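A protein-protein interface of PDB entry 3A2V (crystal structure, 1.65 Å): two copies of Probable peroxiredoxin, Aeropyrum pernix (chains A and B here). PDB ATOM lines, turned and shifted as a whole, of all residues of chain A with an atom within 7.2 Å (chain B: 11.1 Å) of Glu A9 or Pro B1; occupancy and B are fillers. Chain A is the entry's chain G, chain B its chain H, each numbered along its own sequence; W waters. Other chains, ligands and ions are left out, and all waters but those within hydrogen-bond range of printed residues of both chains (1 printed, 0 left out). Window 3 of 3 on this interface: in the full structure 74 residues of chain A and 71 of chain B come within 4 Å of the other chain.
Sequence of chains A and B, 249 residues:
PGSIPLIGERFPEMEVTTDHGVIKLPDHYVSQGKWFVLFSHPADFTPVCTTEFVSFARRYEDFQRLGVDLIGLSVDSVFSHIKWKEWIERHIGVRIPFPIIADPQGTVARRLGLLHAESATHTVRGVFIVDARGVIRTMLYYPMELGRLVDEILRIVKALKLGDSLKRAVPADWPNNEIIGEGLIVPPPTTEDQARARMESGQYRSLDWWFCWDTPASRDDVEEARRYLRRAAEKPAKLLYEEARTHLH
Ile B4 touches its own counterpart, Ile A4. Of the 17 pairs that touch across the chains among the printed residues, 1 has its exchanged pair printed and touching as well.
Glu A9 touches just these residues of chain B: Pro B1 (2.8 Å) and Ala B117 (3.6 Å). Of chain A, only Ser A3, Ile A4, Leu A6 and Glu A9 come within 4 Å of Pro B1. Ser A3 touches just these residues of chain B: Pro B1 (3.6 Å) and Gly B2 (3.3 Å). Leu A6 touches four residues of chain B. Of the printed residues of chain A, Leu B115 touches Leu A6. Of the printed residues of chain A, Ile B4 touches Ile A4. Ala B120 touches none of the printed residues of chain A. The nearest residue of chain B that does not touch Glu A9 is Gly B2 (5.2 Å).
Water W1 lies within hydrogen-bond range of OE1 of Glu B145, NE of Arg A137 and OE1 of Glu B118.
Printed residues of chain A that touch a printed residue of chain B: Ser A3, Ile A4, Leu A6, Ile A7, Gly A8, Glu A9 and Arg A137. Hydrophobic or aromatic side chains of chain B within 4 Å of the printed part of chain A: Pro B1, Ile B4, His B116, Ala B117 and Pro B143.
N of Leu A6 is in hydrogen-bond range of OE2 of Glu A9 (3.1 Å). O of Ile A136 is in hydrogen-bond range of N of Gly A8 (2.8 Å). O of Gly B113 is in hydrogen-bond range of NE2 of His B116, 3.0 Å away. O of Glu A9 sits at hydrogen-bond distance from N of Ile A136.
OG of Ser A3 touches CB of Pro B1 (3.6 Å). Gly B2 touches Ser A3. Pro B1 touches Ile A4 (CA to O, 3.2 Å). Ile B4 touches Ile A4 (CD1 to CG2, 3.5 Å). Leu A6 touches Pro B1. Leu A6 touches Gly B2 (CG to N, 3.8 Å). CD1 of Leu A6 touches O of Leu B115, 3.8 Å away. CB of Leu A6 touches ND1 of His B116 (3.7 Å). CB of Ala B117 touches C of Gly A8, 3.7 Å away. Arg A137 touches Pro B143.
The backbone NH (N) of Ile A4 lies within hydrogen-bond range of the backbone carbonyl oxygen (O) of Gly B2 (2.7 Å). ND1 of His B116 lies within hydrogen-bond range of N of Ile A7 (3.0 Å). The guanidinium group (NH2) of Arg A137 lies within salt-bridge range of the side-chain carboxylate (OE1) of Glu B145. The backbone carbonyl oxygen (O) of Ile A7 is in hydrogen-bond range of the backbone NH (N) of Ala B117 (2.8 Å). The side-chain carboxylate (OE1) of Glu A9 lies close to the backbone nitrogen (N) of Pro B1 (2.8 Å). The backbone carbonyl oxygen (O) of Ile A7 lies within hydrogen-bond range of the backbone NH (N) of Glu B118 (3.4 Å).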
ATOM      1  N   SER A   3      17.654   9.176  14.876  1.00  0.00           N
ATOM      2  CA  SER A   3      17.575   9.307  13.422  1.00  0.00           C
ATOM      3  C   SER A   3      16.215   9.859  13.016  1.00  0.00           C
ATOM      4  O   SER A   3      15.202   9.453  13.567  1.00  0.00           O
ATOM      5  CB  SER A   3      17.798   7.964  12.742  1.00  0.00           C
ATOM      6  OG  SER A   3      17.787   8.121  11.337  1.00  0.00           O
ATOM      7  N   ILE A   4      16.212  10.802  12.071  1.00  0.00           N
ATOM      8  CA  ILE A   4      14.982  11.306  11.465  1.00  0.00           C
ATOM      9  C   ILE A   4      15.133  11.349   9.946  1.00  0.00           C
ATOM     10  O   ILE A   4      16.259  11.426   9.435  1.00  0.00           O
ATOM     11  CB  ILE A   4      14.588  12.727  11.991  1.00  0.00           C
ATOM     12  CG1 ILE A   4      15.674  13.777  11.688  1.00  0.00           C
ATOM     13  CG2 ILE A   4      14.235  12.688  13.481  1.00  0.00           C
ATOM     14  CD1 ILE A   4      15.153  15.243  11.730  1.00  0.00           C
ATOM     15  N   PRO A   5      14.010  11.274   9.214  1.00  0.00           N
ATOM     16  CA  PRO A   5      14.071  11.567   7.775  1.00  0.00           C
ATOM     17  C   PRO A   5      14.366  13.061   7.621  1.00  0.00           C
ATOM     18  O   PRO A   5      14.280  13.808   8.595  1.00  0.00           O
ATOM     19  CB  PRO A   5      12.662  11.236   7.281  1.00  0.00           C
ATOM     20  CG  PRO A   5      11.790  11.303   8.501  1.00  0.00           C
ATOM     21  CD  PRO A   5      12.651  10.919   9.664  1.00  0.00           C
ATOM     22  N   LEU A   6      14.758  13.491   6.424  1.00  0.00           N
ATOM     23  CA  LEU A   6      15.269  14.858   6.263  1.00  0.00           C
ATOM     24  C   LEU A   6      14.522  15.625   5.180  1.00  0.00           C
ATOM     25  O   LEU A   6      13.958  15.028   4.267  1.00  0.00           O
ATOM     26  CB  LEU A   6      16.766  14.829   5.934  1.00  0.00           C
ATOM     27  CG  LEU A   6      17.705  14.127   6.927  1.00  0.00           C
ATOM     28  CD1 LEU A   6      19.111  14.055   6.354  1.00  0.00           C
ATOM     29  CD2 LEU A   6      17.724  14.799   8.306  1.00  0.00           C
ATOM     30  N   ILE A   7      14.516  16.956   5.315  1.00  0.00           N
ATOM     31  CA  ILE A   7      13.934  17.835   4.303  1.00  0.00           C
ATOM     32  C   ILE A   7      14.649  17.555   2.990  1.00  0.00           C
ATOM     33  O   ILE A   7      15.880  17.427   2.954  1.00  0.00           O
ATOM     34  CB  ILE A   7      14.115  19.327   4.684  1.00  0.00           C
ATOM     35  CG1 ILE A   7      13.301  19.695   5.943  1.00  0.00           C
ATOM     36  CG2 ILE A   7      13.776  20.231   3.508  1.00  0.00           C
ATOM     37  CD1 ILE A   7      13.599  21.058   6.484  1.00  0.00           C
ATOM     38  N   GLY A   8      13.870  17.499   1.915  1.00  0.00           N
ATOM     39  CA  GLY A   8      14.380  17.188   0.593  1.00  0.00           C
ATOM     40  C   GLY A   8      14.368  15.718   0.221  1.00  0.00           C
ATOM     41  O   GLY A   8      14.476  15.391  -0.967  1.00  0.00           O
ATOM     42  N   GLU A   9      14.267  14.830   1.213  1.00  0.00           N
ATOM     43  CA  GLU A   9      14.160  13.380   0.963  1.00  0.00           C
ATOM     44  C   GLU A   9      12.715  12.980   0.671  1.00  0.00           C
ATOM     45  O   GLU A   9      11.782  13.544   1.244  1.00  0.00           O
ATOM     46  CB  GLU A   9      14.614  12.574   2.180  1.00  0.00           C
ATOM     47  CG  GLU A   9      16.094  12.609   2.478  1.00  0.00           C
ATOM     48  CD  GLU A   9      16.473  11.726   3.665  1.00  0.00           C
ATOM     49  OE1 GLU A   9      17.685  11.503   3.878  1.00  0.00           O
ATOM     50  OE2 GLU A   9      15.567  11.268   4.398  1.00  0.00           O
ATOM     51  N   ARG A  10      12.522  11.983  -0.188  1.00  0.00           N
ATOM     52  CA  ARG A  10      11.179  11.415  -0.354  1.00  0.00           C
ATOM     53  C   ARG A  10      10.737  10.821   1.003  1.00  0.00           C
ATOM     54  O   ARG A  10      11.558  10.250   1.735  1.00  0.00           O
ATOM     55  CB  ARG A  10      11.162  10.364  -1.477  1.00  0.00           C
ATOM     56  CG  ARG A  10       9.753   9.914  -1.884  1.00  0.00           C
ATOM     57  CD  ARG A  10       9.755   9.146  -3.209  1.00  0.00           C
ATOM     58  NE  ARG A  10       8.411   8.980  -3.777  1.00  0.00           N
ATOM     59  CZ  ARG A  10       7.584   7.973  -3.496  1.00  0.00           C
ATOM     60  NH1 ARG A  10       7.927   7.034  -2.620  1.00  0.00           N
ATOM     61  NH2 ARG A  10       6.395   7.911  -4.084  1.00  0.00           N
ATOM     62  N   PHE A  11       9.461  11.003   1.343  1.00  0.00           N
ATOM     63  CA  PHE A  11       8.897  10.487   2.587  1.00  0.00           C
ATOM     64  C   PHE A  11       9.093   8.958   2.556  1.00  0.00           C
ATOM     65  O   PHE A  11       8.846   8.347   1.515  1.00  0.00           O
ATOM     66  CB  PHE A  11       7.407  10.869   2.687  1.00  0.00           C
ATOM     67  CG  PHE A  11       6.740  10.414   3.946  1.00  0.00           C
ATOM     68  CD1 PHE A  11       6.712  11.234   5.080  1.00  0.00           C
ATOM     69  CD2 PHE A  11       6.156   9.160   4.017  1.00  0.00           C
ATOM     70  CE1 PHE A  11       6.103  10.813   6.245  1.00  0.00           C
ATOM     71  CE2 PHE A  11       5.559   8.723   5.178  1.00  0.00           C
ATOM     72  CZ  PHE A  11       5.534   9.542   6.294  1.00  0.00           C
ATOM     73  N   PRO A  12       9.544   8.349   3.675  1.00  0.00           N
ATOM     74  CA  PRO A  12       9.816   6.910   3.698  1.00  0.00           C
ATOM     75  C   PRO A  12       8.612   6.095   3.226  1.00  0.00           C
ATOM     76  O   PRO A  12       7.498   6.298   3.696  1.00  0.00           O
ATOM     77  CB  PRO A  12      10.110   6.628   5.176  1.00  0.00           C
ATOM     78  CG  PRO A  12      10.600   7.902   5.713  1.00  0.00           C
ATOM     79  CD  PRO A  12       9.852   8.984   4.970  1.00  0.00           C
ATOM     80  N   ARG A 111      10.612   4.890  12.424  1.00  0.00           N
ATOM     81  CA  ARG A 111      11.001   5.242  11.053  1.00  0.00           C
ATOM     82  C   ARG A 111      11.009   6.767  10.846  1.00  0.00           C
ATOM     83  O   ARG A 111      11.827   7.297  10.085  1.00  0.00           O
ATOM     84  CB  ARG A 111      10.043   4.563  10.059  1.00  0.00           C
ATOM     85  CG  ARG A 111      10.491   4.508   8.610  1.00  0.00           C
ATOM     86  CD  ARG A 111      10.972   3.094   8.232  1.00  0.00           C
ATOM     87  NE  ARG A 111      10.482   2.671   6.918  1.00  0.00           N
ATOM     88  CZ  ARG A 111      11.033   3.026   5.761  1.00  0.00           C
ATOM     89  NH1 ARG A 111      12.098   3.823   5.738  1.00  0.00           N
ATOM     90  NH2 ARG A 111      10.521   2.587   4.624  1.00  0.00           N
ATOM     91  N   VAL A 130       4.522  17.336   3.425  1.00  0.00           N
ATOM     92  CA  VAL A 130       4.971  16.497   2.309  1.00  0.00           C
ATOM     93  C   VAL A 130       4.284  16.992   1.042  1.00  0.00           C
ATOM     94  O   VAL A 130       3.074  17.202   1.016  1.00  0.00           O
ATOM     95  CB  VAL A 130       4.659  15.005   2.512  1.00  0.00           C
ATOM     96  CG1 VAL A 130       5.221  14.181   1.375  1.00  0.00           C
ATOM     97  CG2 VAL A 130       5.237  14.497   3.847  1.00  0.00           C
ATOM     98  N   GLY A 134       5.817  13.770  -3.065  1.00  0.00           N
ATOM     99  CA  GLY A 134       6.155  12.905  -1.944  1.00  0.00           C
ATOM    100  C   GLY A 134       7.385  13.343  -1.153  1.00  0.00           C
ATOM    101  O   GLY A 134       7.890  12.565  -0.342  1.00  0.00           O
ATOM    102  N   VAL A 135       7.859  14.577  -1.367  1.00  0.00           N
ATOM    103  CA  VAL A 135       9.093  15.060  -0.719  1.00  0.00           C
ATOM    104  C   VAL A 135       8.790  15.820   0.577  1.00  0.00           C
ATOM    105  O   VAL A 135       7.894  16.657   0.598  1.00  0.00           O
ATOM    106  CB  VAL A 135       9.924  15.975  -1.686  1.00  0.00           C
ATOM    107  CG1 VAL A 135      11.162  16.515  -1.005  1.00  0.00           C
ATOM    108  CG2 VAL A 135      10.279  15.192  -2.945  1.00  0.00           C
ATOM    109  N   ILE A 136       9.537  15.508   1.640  1.00  0.00           N
ATOM    110  CA  ILE A 136       9.440  16.204   2.925  1.00  0.00           C
ATOM    111  C   ILE A 136       9.944  17.636   2.721  1.00  0.00           C
ATOM    112  O   ILE A 136      11.073  17.849   2.239  1.00  0.00           O
ATOM    113  CB  ILE A 136      10.249  15.469   4.032  1.00  0.00           C
ATOM    114  CG1 ILE A 136       9.679  14.050   4.236  1.00  0.00           C
ATOM    115  CG2 ILE A 136      10.207  16.244   5.357  1.00  0.00           C
ATOM    116  CD1 ILE A 136      10.598  13.137   5.078  1.00  0.00           C
ATOM    117  N   ARG A 137       9.112  18.599   3.102  1.00  0.00           N
ATOM    118  CA  ARG A 137       9.418  20.004   2.893  1.00  0.00           C
ATOM    119  C   ARG A 137       9.691  20.824   4.152  1.00  0.00           C
ATOM    120  O   ARG A 137      10.308  21.877   4.063  1.00  0.00           O
ATOM    121  CB  ARG A 137       8.300  20.676   2.084  1.00  0.00           C
ATOM    122  CG  ARG A 137       7.942  19.999   0.719  1.00  0.00           C
ATOM    123  CD  ARG A 137       9.134  20.084  -0.258  1.00  0.00           C
ATOM    124  NE  ARG A 137       9.404  21.496  -0.553  1.00  0.00           N
ATOM    125  CZ  ARG A 137       8.764  22.222  -1.473  1.00  0.00           C
ATOM    126  NH1 ARG A 137       7.835  21.668  -2.273  1.00  0.00           N
ATOM    127  NH2 ARG A 137       9.069  23.513  -1.598  1.00  0.00           N
ATOM    128  N   PRO B   1      18.062   9.394   5.727  1.00  0.00           N
ATOM    129  CA  PRO B   1      17.810   9.984   7.032  1.00  0.00           C
ATOM    130  C   PRO B   1      19.081  10.554   7.670  1.00  0.00           C
ATOM    131  O   PRO B   1      20.158  10.474   7.083  1.00  0.00           O
ATOM    132  CB  PRO B   1      17.289   8.800   7.853  1.00  0.00           C
ATOM    133  CG  PRO B   1      16.634   7.914   6.868  1.00  0.00           C
ATOM    134  CD  PRO B   1      17.313   8.138   5.532  1.00  0.00           C
ATOM    135  N   GLY B   2      18.944  11.124   8.865  1.00  0.00           N
ATOM    136  CA  GLY B   2      20.090  11.671   9.583  1.00  0.00           C
ATOM    137  C   GLY B   2      19.841  11.789  11.070  1.00  0.00           C
ATOM    138  O   GLY B   2      18.699  11.793  11.520  1.00  0.00           O
ATOM    139  N   SER B   3      20.919  11.893  11.833  1.00  0.00           N
ATOM    140  CA  SER B   3      20.827  11.901  13.282  1.00  0.00           C
ATOM    141  C   SER B   3      20.634  13.327  13.816  1.00  0.00           C
ATOM    142  O   SER B   3      21.270  14.271  13.342  1.00  0.00           O
ATOM    143  CB  SER B   3      22.067  11.241  13.889  1.00  0.00           C
ATOM    144  OG  SER B   3      22.026  11.309  15.302  1.00  0.00           O
ATOM    145  N   ILE B   4      19.732  13.479  14.782  1.00  0.00           N
ATOM    146  CA  ILE B   4      19.524  14.756  15.445  1.00  0.00           C
ATOM    147  C   ILE B   4      19.546  14.596  16.965  1.00  0.00           C
ATOM    148  O   ILE B   4      19.252  13.498  17.499  1.00  0.00           O
ATOM    149  CB  ILE B   4      18.177  15.435  15.024  1.00  0.00           C
ATOM    150  CG1 ILE B   4      16.973  14.529  15.342  1.00  0.00           C
ATOM    151  CG2 ILE B   4      18.221  15.860  13.562  1.00  0.00           C
ATOM    152  CD1 ILE B   4      15.624  15.272  15.450  1.00  0.00           C
ATOM    153  N   ARG B 110      26.710  19.195  11.677  1.00  0.00           N
ATOM    154  CA  ARG B 110      26.616  17.731  11.693  1.00  0.00           C
ATOM    155  C   ARG B 110      26.166  17.214  13.037  1.00  0.00           C
ATOM    156  O   ARG B 110      25.294  16.336  13.109  1.00  0.00           O
ATOM    157  CB  ARG B 110      27.965  17.095  11.342  1.00  0.00           C
ATOM    158  CG  ARG B 110      28.308  17.141   9.884  1.00  0.00           C
ATOM    159  CD  ARG B 110      29.677  16.494   9.658  1.00  0.00           C
ATOM    160  NE  ARG B 110      30.462  17.276   8.709  1.00  0.00           N
ATOM    161  CZ  ARG B 110      31.664  17.795   8.947  1.00  0.00           C
ATOM    162  NH1 ARG B 110      32.281  17.616  10.117  1.00  0.00           N
ATOM    163  NH2 ARG B 110      32.267  18.477   7.981  1.00  0.00           N
ATOM    164  N   LEU B 112      24.367  18.720  15.137  1.00  0.00           N
ATOM    165  CA  LEU B 112      22.992  19.131  15.401  1.00  0.00           C
ATOM    166  C   LEU B 112      21.957  18.646  14.380  1.00  0.00           C
ATOM    167  O   LEU B 112      20.755  18.925  14.512  1.00  0.00           O
ATOM    168  CB  LEU B 112      22.931  20.655  15.587  1.00  0.00           C
ATOM    169  CG  LEU B 112      23.724  21.248  16.761  1.00  0.00           C
ATOM    170  CD1 LEU B 112      23.591  22.744  16.795  1.00  0.00           C
ATOM    171  CD2 LEU B 112      23.312  20.630  18.127  1.00  0.00           C
ATOM    172  N   GLY B 113      22.437  17.909  13.385  1.00  0.00           N
ATOM    173  CA  GLY B 113      21.617  17.275  12.375  1.00  0.00           C
ATOM    174  C   GLY B 113      21.087  18.281  11.380  1.00  0.00           C
ATOM    175  O   GLY B 113      19.990  18.111  10.852  1.00  0.00           O
ATOM    176  N   LEU B 114      21.869  19.337  11.135  1.00  0.00           N
ATOM    177  CA  LEU B 114      21.358  20.512  10.401  1.00  0.00           C
ATOM    178  C   LEU B 114      21.634  20.448   8.904  1.00  0.00           C
ATOM    179  O   LEU B 114      21.250  21.346   8.140  1.00  0.00           O
ATOM    180  CB  LEU B 114      21.896  21.807  11.005  1.00  0.00           C
ATOM    181  CG  LEU B 114      21.378  22.158  12.407  1.00  0.00           C
ATOM    182  CD1 LEU B 114      22.160  23.326  12.999  1.00  0.00           C
ATOM    183  CD2 LEU B 114      19.858  22.501  12.374  1.00  0.00           C
ATOM    184  N   LEU B 115      22.289  19.375   8.487  1.00  0.00           N
ATOM    185  CA  LEU B 115      22.483  19.144   7.072  1.00  0.00           C
ATOM    186  C   LEU B 115      21.448  18.143   6.539  1.00  0.00           C
ATOM    187  O   LEU B 115      21.489  16.937   6.840  1.00  0.00           O
ATOM    188  CB  LEU B 115      23.929  18.712   6.800  1.00  0.00           C
ATOM    189  CG  LEU B 115      24.951  19.794   7.180  1.00  0.00           C
ATOM    190  CD1 LEU B 115      26.328  19.184   7.407  1.00  0.00           C
ATOM    191  CD2 LEU B 115      25.033  20.890   6.129  1.00  0.00           C
ATOM    192  N   HIS B 116      20.511  18.649   5.746  1.00  0.00           N
ATOM    193  CA  HIS B 116      19.453  17.811   5.220  1.00  0.00           C
ATOM    194  C   HIS B 116      19.684  17.591   3.724  1.00  0.00           C
ATOM    195  O   HIS B 116      20.755  17.946   3.208  1.00  0.00           O
ATOM    196  CB  HIS B 116      18.088  18.442   5.505  1.00  0.00           C
ATOM    197  CG  HIS B 116      17.688  18.394   6.951  1.00  0.00           C
ATOM    198  ND1 HIS B 116      16.386  18.171   7.352  1.00  0.00           N
ATOM    199  CD2 HIS B 116      18.417  18.531   8.088  1.00  0.00           C
ATOM    200  CE1 HIS B 116      16.328  18.190   8.676  1.00  0.00           C
ATOM    201  NE2 HIS B 116      17.545  18.412   9.147  1.00  0.00           N
ATOM    202  N   ALA B 117      18.696  17.014   3.042  1.00  0.00           N
ATOM    203  CA  ALA B 117      18.852  16.583   1.644  1.00  0.00           C
ATOM    204  C   ALA B 117      18.730  17.684   0.598  1.00  0.00           C
ATOM    205  O   ALA B 117      19.086  17.451  -0.557  1.00  0.00           O
ATOM    206  CB  ALA B 117      17.903  15.439   1.317  1.00  0.00           C
ATOM    207  N   GLU B 118      18.219  18.864   0.955  1.00  0.00           N
ATOM    208  CA  GLU B 118      18.115  19.901  -0.076  1.00  0.00           C
ATOM    209  C   GLU B 118      19.469  20.499  -0.472  1.00  0.00           C
ATOM    210  O   GLU B 118      19.658  20.899  -1.628  1.00  0.00           O
ATOM    211  CB  GLU B 118      17.036  20.971   0.184  1.00  0.00           C
ATOM    212  CG  GLU B 118      16.837  21.471   1.601  1.00  0.00           C
ATOM    213  CD  GLU B 118      15.807  22.639   1.680  1.00  0.00           C
ATOM    214  OE1 GLU B 118      14.828  22.672   0.864  1.00  0.00           O
ATOM    215  OE2 GLU B 118      16.009  23.513   2.558  1.00  0.00           O
ATOM    216  N   SER B 119      20.416  20.489   0.465  1.00  0.00           N
ATOM    217  CA  SER B 119      21.757  21.007   0.221  1.00  0.00           C
ATOM    218  C   SER B 119      22.809  20.182   0.959  1.00  0.00           C
ATOM    219  O   SER B 119      22.696  19.924   2.164  1.00  0.00           O
ATOM    220  CB  SER B 119      21.855  22.477   0.643  1.00  0.00           C
ATOM    221  OG  SER B 119      23.201  22.941   0.591  1.00  0.00           O
ATOM    222  N   ALA B 120      23.851  19.790   0.230  1.00  0.00           N
ATOM    223  CA  ALA B 120      24.966  19.055   0.829  1.00  0.00           C
ATOM    224  C   ALA B 120      25.846  19.992   1.622  1.00  0.00           C
ATOM    225  O   ALA B 120      26.654  19.566   2.445  1.00  0.00           O
ATOM    226  CB  ALA B 120      25.787  18.383  -0.259  1.00  0.00           C
ATOM    227  N   VAL B 124      19.917  23.732   6.938  1.00  0.00           N
ATOM    228  CA  VAL B 124      18.530  24.168   6.854  1.00  0.00           C
ATOM    229  C   VAL B 124      18.300  25.266   7.908  1.00  0.00           C
ATOM    230  O   VAL B 124      19.243  25.726   8.582  1.00  0.00           O
ATOM    231  CB  VAL B 124      17.560  22.975   7.129  1.00  0.00           C
ATOM    232  CG1 VAL B 124      17.526  22.004   5.914  1.00  0.00           C
ATOM    233  CG2 VAL B 124      17.950  22.301   8.418  1.00  0.00           C
ATOM    234  N   PRO B 143      12.799  25.063   5.700  1.00  0.00           N
ATOM    235  CA  PRO B 143      13.652  24.842   4.547  1.00  0.00           C
ATOM    236  C   PRO B 143      14.244  26.138   3.980  1.00  0.00           C
ATOM    237  O   PRO B 143      13.899  27.223   4.462  1.00  0.00           O
ATOM    238  CB  PRO B 143      12.687  24.229   3.553  1.00  0.00           C
ATOM    239  CG  PRO B 143      11.368  24.933   3.814  1.00  0.00           C
ATOM    240  CD  PRO B 143      11.392  25.282   5.326  1.00  0.00           C
ATOM    241  N   GLU B 145      13.762  27.762   1.348  1.00  0.00           N
ATOM    242  CA  GLU B 145      12.895  28.650   0.569  1.00  0.00           C
ATOM    243  C   GLU B 145      11.823  29.337   1.389  1.00  0.00           C
ATOM    244  O   GLU B 145      10.981  30.071   0.836  1.00  0.00           O
ATOM    245  CB  GLU B 145      12.251  27.857  -0.576  1.00  0.00           C
ATOM    246  CG  GLU B 145      11.290  26.722  -0.121  1.00  0.00           C
ATOM    247  CD  GLU B 145      11.945  25.348   0.099  1.00  0.00           C
ATOM    248  OE1 GLU B 145      11.212  24.329   0.073  1.00  0.00           O
ATOM    249  OE2 GLU B 145      13.174  25.254   0.280  1.00  0.00           O
HETATM  250  O   HOH W   1      11.451  22.152   1.353  1.00  0.00           O
